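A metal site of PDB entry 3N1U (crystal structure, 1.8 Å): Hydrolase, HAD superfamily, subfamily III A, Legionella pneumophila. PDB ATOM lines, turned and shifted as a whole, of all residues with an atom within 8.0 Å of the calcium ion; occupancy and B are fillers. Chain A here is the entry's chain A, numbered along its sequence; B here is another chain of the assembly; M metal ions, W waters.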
ATOM      1  N   ASP A  25     -14.296 -14.972   8.901  1.00  0.00           N
ATOM      2  CA  ASP A  25     -14.162 -13.685   8.221  1.00  0.00           C
ATOM      3  C   ASP A  25     -12.945 -13.788   7.275  1.00  0.00           C
ATOM      4  O   ASP A  25     -12.119 -14.706   7.420  1.00  0.00           O
ATOM      5  CB  ASP A  25     -13.895 -12.614   9.257  1.00  0.00           C
ATOM      6  CG  ASP A  25     -13.672 -11.244   8.625  1.00  0.00           C
ATOM      7  OD1 ASP A  25     -14.408 -10.856   7.688  1.00  0.00           O
ATOM      8  OD2 ASP A  25     -12.761 -10.556   9.085  1.00  0.00           O
ATOM      9  N   VAL A  26     -12.847 -12.879   6.298  1.00  0.00           N
ATOM     10  CA  VAL A  26     -11.686 -12.869   5.391  1.00  0.00           C
ATOM     11  C   VAL A  26     -10.551 -11.966   5.845  1.00  0.00           C
ATOM     12  O   VAL A  26      -9.557 -12.426   6.417  1.00  0.00           O
ATOM     13  CB  VAL A  26     -12.110 -12.535   3.930  1.00  0.00           C
ATOM     14  CG1 VAL A  26     -10.861 -12.488   3.034  1.00  0.00           C
ATOM     15  CG2 VAL A  26     -13.118 -13.630   3.469  1.00  0.00           C
ATOM     16  N   ASP A  27     -10.695 -10.643   5.668  1.00  0.00           N
ATOM     17  CA  ASP A  27      -9.551  -9.772   5.832  1.00  0.00           C
ATOM     18  C   ASP A  27      -9.167  -9.657   7.296  1.00  0.00           C
ATOM     19  O   ASP A  27     -10.023  -9.273   8.090  1.00  0.00           O
ATOM     20  CB  ASP A  27      -9.933  -8.364   5.346  1.00  0.00           C
ATOM     21  CG  ASP A  27     -10.157  -8.320   3.845  1.00  0.00           C
ATOM     22  OD1 ASP A  27      -9.154  -8.374   3.091  1.00  0.00           O
ATOM     23  OD2 ASP A  27     -11.299  -8.234   3.428  1.00  0.00           O
ATOM     24  N   GLY A  28      -7.922  -9.996   7.643  1.00  0.00           N
ATOM     25  CA  GLY A  28      -7.482  -9.940   9.063  1.00  0.00           C
ATOM     26  C   GLY A  28      -7.571 -11.303   9.763  1.00  0.00           C
ATOM     27  O   GLY A  28      -7.035 -11.499  10.905  1.00  0.00           O
ATOM     28  N   VAL A  29      -8.253 -12.249   9.112  1.00  0.00           N
ATOM     29  CA  VAL A  29      -8.481 -13.588   9.686  1.00  0.00           C
ATOM     30  C   VAL A  29      -7.942 -14.684   8.762  1.00  0.00           C
ATOM     31  O   VAL A  29      -7.042 -15.423   9.139  1.00  0.00           O
ATOM     32  CB  VAL A  29      -9.994 -13.815  10.060  1.00  0.00           C
ATOM     33  CG1 VAL A  29     -10.285 -15.313  10.477  1.00  0.00           C
ATOM     34  CG2 VAL A  29     -10.439 -12.838  11.184  1.00  0.00           C
ATOM     35  N   LEU A  30      -8.460 -14.755   7.541  1.00  0.00           N
ATOM     36  CA  LEU A  30      -7.838 -15.603   6.539  1.00  0.00           C
ATOM     37  C   LEU A  30      -6.657 -14.871   5.860  1.00  0.00           C
ATOM     38  O   LEU A  30      -5.809 -15.499   5.238  1.00  0.00           O
ATOM     39  CB  LEU A  30      -8.896 -16.034   5.513  1.00  0.00           C
ATOM     40  CG  LEU A  30      -9.860 -17.143   6.085  1.00  0.00           C
ATOM     41  CD1 LEU A  30     -11.028 -17.303   5.122  1.00  0.00           C
ATOM     42  CD2 LEU A  30      -9.132 -18.500   6.217  1.00  0.00           C
ATOM     43  N   SER A  31      -6.594 -13.531   6.023  1.00  0.00           N
ATOM     44  CA  SER A  31      -5.412 -12.772   5.619  1.00  0.00           C
ATOM     45  C   SER A  31      -4.751 -12.128   6.795  1.00  0.00           C
ATOM     46  O   SER A  31      -5.364 -12.073   7.898  1.00  0.00           O
ATOM     47  CB  SER A  31      -5.814 -11.707   4.595  1.00  0.00           C
ATOM     48  OG  SER A  31      -6.450 -10.585   5.246  1.00  0.00           O
ATOM     49  N   GLY A  33      -4.540  -9.145   6.998  1.00  0.00           N
ATOM     50  CA  GLY A  33      -5.149  -7.800   7.155  1.00  0.00           C
ATOM     51  C   GLY A  33      -4.744  -6.811   6.079  1.00  0.00           C
ATOM     52  O   GLY A  33      -5.286  -5.728   6.008  1.00  0.00           O
ATOM     53  N   ILE A  68     -18.097 -15.141   5.916  1.00  0.00           N
ATOM     54  CA  ILE A  68     -18.949 -13.927   5.907  1.00  0.00           C
ATOM     55  C   ILE A  68     -17.980 -12.756   5.959  1.00  0.00           C
ATOM     56  O   ILE A  68     -17.219 -12.584   6.935  1.00  0.00           O
ATOM     57  CB  ILE A  68     -19.956 -13.841   7.106  1.00  0.00           C
ATOM     58  CG1 ILE A  68     -20.858 -15.064   7.155  1.00  0.00           C
ATOM     59  CG2 ILE A  68     -20.775 -12.525   7.027  1.00  0.00           C
ATOM     60  CD1 ILE A  68     -21.859 -15.091   8.338  1.00  0.00           C
ATOM     61  N   THR A  69     -18.001 -11.957   4.909  1.00  0.00           N
ATOM     62  CA  THR A  69     -16.988 -10.888   4.800  1.00  0.00           C
ATOM     63  C   THR A  69     -17.612  -9.569   4.351  1.00  0.00           C
ATOM     64  O   THR A  69     -18.640  -9.572   3.629  1.00  0.00           O
ATOM     65  CB  THR A  69     -15.835 -11.290   3.794  1.00  0.00           C
ATOM     66  OG1 THR A  69     -14.923 -10.196   3.716  1.00  0.00           O
ATOM     67  CG2 THR A  69     -16.382 -11.538   2.402  1.00  0.00           C
ATOM     68  N   THR A  70     -16.971  -8.457   4.772  1.00  0.00           N
ATOM     69  CA  THR A  70     -17.273  -7.127   4.222  1.00  0.00           C
ATOM     70  C   THR A  70     -16.613  -6.904   2.845  1.00  0.00           C
ATOM     71  O   THR A  70     -17.141  -6.136   2.010  1.00  0.00           O
ATOM     72  CB  THR A  70     -16.875  -6.018   5.225  1.00  0.00           C
ATOM     73  OG1 THR A  70     -17.546  -6.293   6.473  1.00  0.00           O
ATOM     74  CG2 THR A  70     -17.308  -4.587   4.703  1.00  0.00           C
ATOM     75  N   ALA A  71     -15.492  -7.608   2.598  1.00  0.00           N
ATOM     76  CA  ALA A  71     -14.802  -7.530   1.300  1.00  0.00           C
ATOM     77  C   ALA A  71     -15.793  -7.862   0.161  1.00  0.00           C
ATOM     78  O   ALA A  71     -16.681  -8.699   0.336  1.00  0.00           O
ATOM     79  CB  ALA A  71     -13.545  -8.482   1.266  1.00  0.00           C
ATOM     80  N   LYS A  95     -23.137  -8.074   9.690  1.00  0.00           N
ATOM     81  CA  LYS A  95     -23.017  -9.512   9.358  1.00  0.00           C
ATOM     82  C   LYS A  95     -24.146 -10.394   9.921  1.00  0.00           C
ATOM     83  O   LYS A  95     -24.232 -11.578   9.594  1.00  0.00           O
ATOM     84  CB  LYS A  95     -21.665 -10.040   9.851  1.00  0.00           C
ATOM     85  CG  LYS A  95     -20.441  -9.353   9.143  1.00  0.00           C
ATOM     86  CD  LYS A  95     -19.120 -10.055   9.498  1.00  0.00           C
ATOM     87  CE  LYS A  95     -17.972  -9.507   8.618  1.00  0.00           C
ATOM     88  NZ  LYS A  95     -16.694 -10.175   8.947  1.00  0.00           N
ATOM     89  N   TYR A 115     -17.159 -19.285  15.003  1.00  0.00           N
ATOM     90  CA  TYR A 115     -16.931 -18.083  14.213  1.00  0.00           C
ATOM     91  C   TYR A 115     -15.609 -17.472  14.662  1.00  0.00           C
ATOM     92  O   TYR A 115     -15.344 -17.336  15.891  1.00  0.00           O
ATOM     93  CB  TYR A 115     -18.065 -17.037  14.453  1.00  0.00           C
ATOM     94  CG  TYR A 115     -17.920 -15.853  13.517  1.00  0.00           C
ATOM     95  CD1 TYR A 115     -16.944 -14.864  13.723  1.00  0.00           C
ATOM     96  CD2 TYR A 115     -18.719 -15.736  12.388  1.00  0.00           C
ATOM     97  CE1 TYR A 115     -16.822 -13.785  12.844  1.00  0.00           C
ATOM     98  CE2 TYR A 115     -18.607 -14.676  11.530  1.00  0.00           C
ATOM     99  CZ  TYR A 115     -17.652 -13.699  11.762  1.00  0.00           C
ATOM    100  OH  TYR A 115     -17.560 -12.670  10.864  1.00  0.00           O
ATOM    101  N   ILE A 116     -14.748 -17.173  13.698  1.00  0.00           N
ATOM    102  CA  ILE A 116     -13.444 -16.580  13.951  1.00  0.00           C
ATOM    103  C   ILE A 116     -13.355 -15.194  13.243  1.00  0.00           C
ATOM    104  O   ILE A 116     -13.599 -15.058  12.031  1.00  0.00           O
ATOM    105  CB  ILE A 116     -12.275 -17.565  13.635  1.00  0.00           C
ATOM    106  CG1 ILE A 116     -10.922 -16.946  14.044  1.00  0.00           C
ATOM    107  CG2 ILE A 116     -12.305 -18.003  12.125  1.00  0.00           C
ATOM    108  CD1 ILE A 116      -9.730 -17.962  13.959  1.00  0.00           C
ATOM    109  N   GLY A 117     -13.048 -14.192  14.061  1.00  0.00           N
ATOM    110  CA  GLY A 117     -13.198 -12.791  13.664  1.00  0.00           C
ATOM    111  C   GLY A 117     -12.013 -11.966  14.157  1.00  0.00           C
ATOM    112  O   GLY A 117     -11.223 -12.420  14.987  1.00  0.00           O
ATOM    113  N   ASP A 118     -11.931 -10.714  13.708  1.00  0.00           N
ATOM    114  CA  ASP A 118     -10.879  -9.787  14.220  1.00  0.00           C
ATOM    115  C   ASP A 118     -11.355  -8.338  14.550  1.00  0.00           C
ATOM    116  O   ASP A 118     -10.605  -7.565  15.161  1.00  0.00           O
ATOM    117  CB  ASP A 118      -9.747  -9.695  13.185  1.00  0.00           C
ATOM    118  CG  ASP A 118     -10.117  -8.819  11.992  1.00  0.00           C
ATOM    119  OD1 ASP A 118     -11.114  -9.088  11.250  1.00  0.00           O
ATOM    120  OD2 ASP A 118      -9.335  -7.862  11.747  1.00  0.00           O
ATOM    121  N   ASP A 119     -12.576  -7.941  14.120  1.00  0.00           N
ATOM    122  CA  ASP A 119     -12.961  -6.515  14.244  1.00  0.00           C
ATOM    123  C   ASP A 119     -14.441  -6.374  14.705  1.00  0.00           C
ATOM    124  O   ASP A 119     -15.165  -7.391  14.821  1.00  0.00           O
ATOM    125  CB  ASP A 119     -12.640  -5.701  12.951  1.00  0.00           C
ATOM    126  CG  ASP A 119     -12.270  -4.221  13.242  1.00  0.00           C
ATOM    127  OD1 ASP A 119     -12.759  -3.663  14.245  1.00  0.00           O
ATOM    128  OD2 ASP A 119     -11.496  -3.613  12.455  1.00  0.00           O
ATOM    129  N   LEU A 120     -14.868  -5.160  15.003  1.00  0.00           N
ATOM    130  CA  LEU A 120     -16.141  -4.948  15.707  1.00  0.00           C
ATOM    131  C   LEU A 120     -17.356  -5.543  14.999  1.00  0.00           C
ATOM    132  O   LEU A 120     -18.259  -5.999  15.674  1.00  0.00           O
ATOM    133  CB  LEU A 120     -16.335  -3.438  15.985  1.00  0.00           C
ATOM    134  CG  LEU A 120     -15.107  -2.817  16.693  1.00  0.00           C
ATOM    135  CD1 LEU A 120     -15.372  -1.307  16.813  1.00  0.00           C
ATOM    136  CD2 LEU A 120     -14.959  -3.422  18.085  1.00  0.00           C
ATOM    137  N   PRO A 121     -17.397  -5.536  13.650  1.00  0.00           N
ATOM    138  CA  PRO A 121     -18.605  -6.149  13.033  1.00  0.00           C
ATOM    139  C   PRO A 121     -18.736  -7.663  13.224  1.00  0.00           C
ATOM    140  O   PRO A 121     -19.845  -8.214  13.077  1.00  0.00           O
ATOM    141  CB  PRO A 121     -18.519  -5.750  11.559  1.00  0.00           C
ATOM    142  CG  PRO A 121     -17.468  -4.518  11.552  1.00  0.00           C
ATOM    143  CD  PRO A 121     -16.504  -4.925  12.631  1.00  0.00           C
ATOM    144  N   ASP A 122     -17.650  -8.317  13.641  1.00  0.00           N
ATOM    145  CA  ASP A 122     -17.675  -9.747  14.000  1.00  0.00           C
ATOM    146  C   ASP A 122     -18.220  -9.992  15.404  1.00  0.00           C
ATOM    147  O   ASP A 122     -18.613 -11.108  15.739  1.00  0.00           O
ATOM    148  CB  ASP A 122     -16.266 -10.334  13.904  1.00  0.00           C
ATOM    149  CG  ASP A 122     -15.637 -10.166  12.540  1.00  0.00           C
ATOM    150  OD1 ASP A 122     -16.281 -10.480  11.504  1.00  0.00           O
ATOM    151  OD2 ASP A 122     -14.469  -9.693  12.493  1.00  0.00           O
ATOM    152  N   VAL A 135      -8.788 -14.030  16.432  1.00  0.00           N
ATOM    153  CA  VAL A 135      -7.331 -14.120  16.047  1.00  0.00           C
ATOM    154  C   VAL A 135      -6.505 -13.283  17.031  1.00  0.00           C
ATOM    155  O   VAL A 135      -7.035 -12.351  17.682  1.00  0.00           O
ATOM    156  CB  VAL A 135      -7.061 -13.691  14.566  1.00  0.00           C
ATOM    157  CG1 VAL A 135      -7.779 -14.688  13.594  1.00  0.00           C
ATOM    158  CG2 VAL A 135      -7.503 -12.228  14.281  1.00  0.00           C
ATOM    159  N   HIS B  48      -3.724  -1.596   5.899  1.00  0.00           N
ATOM    160  CA  HIS B  48      -4.272  -2.583   6.796  1.00  0.00           C
ATOM    161  C   HIS B  48      -5.760  -2.285   7.016  1.00  0.00           C
ATOM    162  O   HIS B  48      -6.157  -1.148   7.266  1.00  0.00           O
ATOM    163  CB  HIS B  48      -3.506  -2.540   8.132  1.00  0.00           C
ATOM    164  CG  HIS B  48      -3.772  -3.747   8.984  1.00  0.00           C
ATOM    165  ND1 HIS B  48      -4.992  -3.951   9.654  1.00  0.00           N
ATOM    166  CD2 HIS B  48      -3.021  -4.840   9.225  1.00  0.00           C
ATOM    167  CE1 HIS B  48      -4.946  -5.121  10.266  1.00  0.00           C
ATOM    168  NE2 HIS B  48      -3.768  -5.688  10.018  1.00  0.00           N
ATOM    169  N   VAL B  49      -6.573  -3.310   6.927  1.00  0.00           N
ATOM    170  CA  VAL B  49      -8.027  -3.131   7.103  1.00  0.00           C
ATOM    171  C   VAL B  49      -8.445  -2.570   8.452  1.00  0.00           C
ATOM    172  O   VAL B  49      -9.480  -1.924   8.553  1.00  0.00           O
ATOM    173  CB  VAL B  49      -8.785  -4.442   6.880  1.00  0.00           C
ATOM    174  CG1 VAL B  49      -8.751  -4.770   5.355  1.00  0.00           C
ATOM    175  CG2 VAL B  49      -8.281  -5.572   7.815  1.00  0.00           C
ATOM    176  N   GLN B  50      -7.713  -2.890   9.523  1.00  0.00           N
ATOM    177  CA  GLN B  50      -8.130  -2.307  10.822  1.00  0.00           C
ATOM    178  C   GLN B  50      -7.906  -0.802  10.865  1.00  0.00           C
ATOM    179  O   GLN B  50      -8.586  -0.103  11.572  1.00  0.00           O
ATOM    180  CB  GLN B  50      -7.429  -2.956  12.020  1.00  0.00           C
ATOM    181  CG  GLN B  50      -7.878  -4.430  12.233  1.00  0.00           C
ATOM    182  CD  GLN B  50      -7.034  -5.171  13.285  1.00  0.00           C
ATOM    183  OE1 GLN B  50      -6.190  -4.543  13.915  1.00  0.00           O
ATOM    184  NE2 GLN B  50      -7.251  -6.481  13.442  1.00  0.00           N
ATOM    185  N   MET B  53     -10.772   0.808   8.904  1.00  0.00           N
ATOM    186  CA  MET B  53     -11.948   0.852   9.790  1.00  0.00           C
ATOM    187  C   MET B  53     -11.811   1.984  10.839  1.00  0.00           C
ATOM    188  O   MET B  53     -12.791   2.676  11.108  1.00  0.00           O
ATOM    189  CB  MET B  53     -12.146  -0.514  10.489  1.00  0.00           C
ATOM    190  CG  MET B  53     -13.162  -0.527  11.584  1.00  0.00           C
ATOM    191  SD  MET B  53     -14.950  -0.353  10.766  1.00  0.00           S
ATOM    192  CE  MET B  53     -14.990  -2.157  10.142  1.00  0.00           C
HETATM  193 CA    CA M   1     -11.924  -8.539   9.297  1.00  0.00          CA
HETATM  194  O   HOH W   1     -14.032  -7.952  10.368  1.00  0.00           O
HETATM  195  O   HOH W   2     -12.847  -7.319   7.446  1.00  0.00           O
HETATM  196  O   HOH W   3     -10.748  -6.514   9.842  1.00  0.00           O
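Three residues have an atom within 4 Å of the calcium ion: Asp 25, Asp 27 and Asp 118. The nearest printed residue that does not touch the calcium ion is Asp 122 (4.2 Å).
The calcium ion is bound by the side-chain carboxylate (OD1) of Asp 118 (2.2 Å). The calcium ion is bound by OD2 of Asp 25 (2.2 Å). The backbone carbonyl oxygen (O) of Asp 27 binds the calcium ion, 2.4 Å away. Water W2 binds the calcium ion. Water W3 binds the calcium ion, 2.4 Å away. Water W1 binds the calcium ion, 2.4 Å away.
The side-chain carboxylate (OD2) of Asp 122 sits at hydrogen-bond distance from the backbone NH (N) of Asp 118 (3.0 Å). The side-chain amide nitrogen (NE2) of Gln 50 of chain B lies within hydrogen-bond range of the side-chain carboxylate (OD2) of Asp 118 (3.0 Å). NZ of Lys 95 is in salt-bridge range of OD1 of Asp 25 (2.7 Å). The backbone NH (N) of Asp 25 is in hydrogen-bond range of the backbone carbonyl oxygen (O) of Ile 116, 3.2 Å away.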
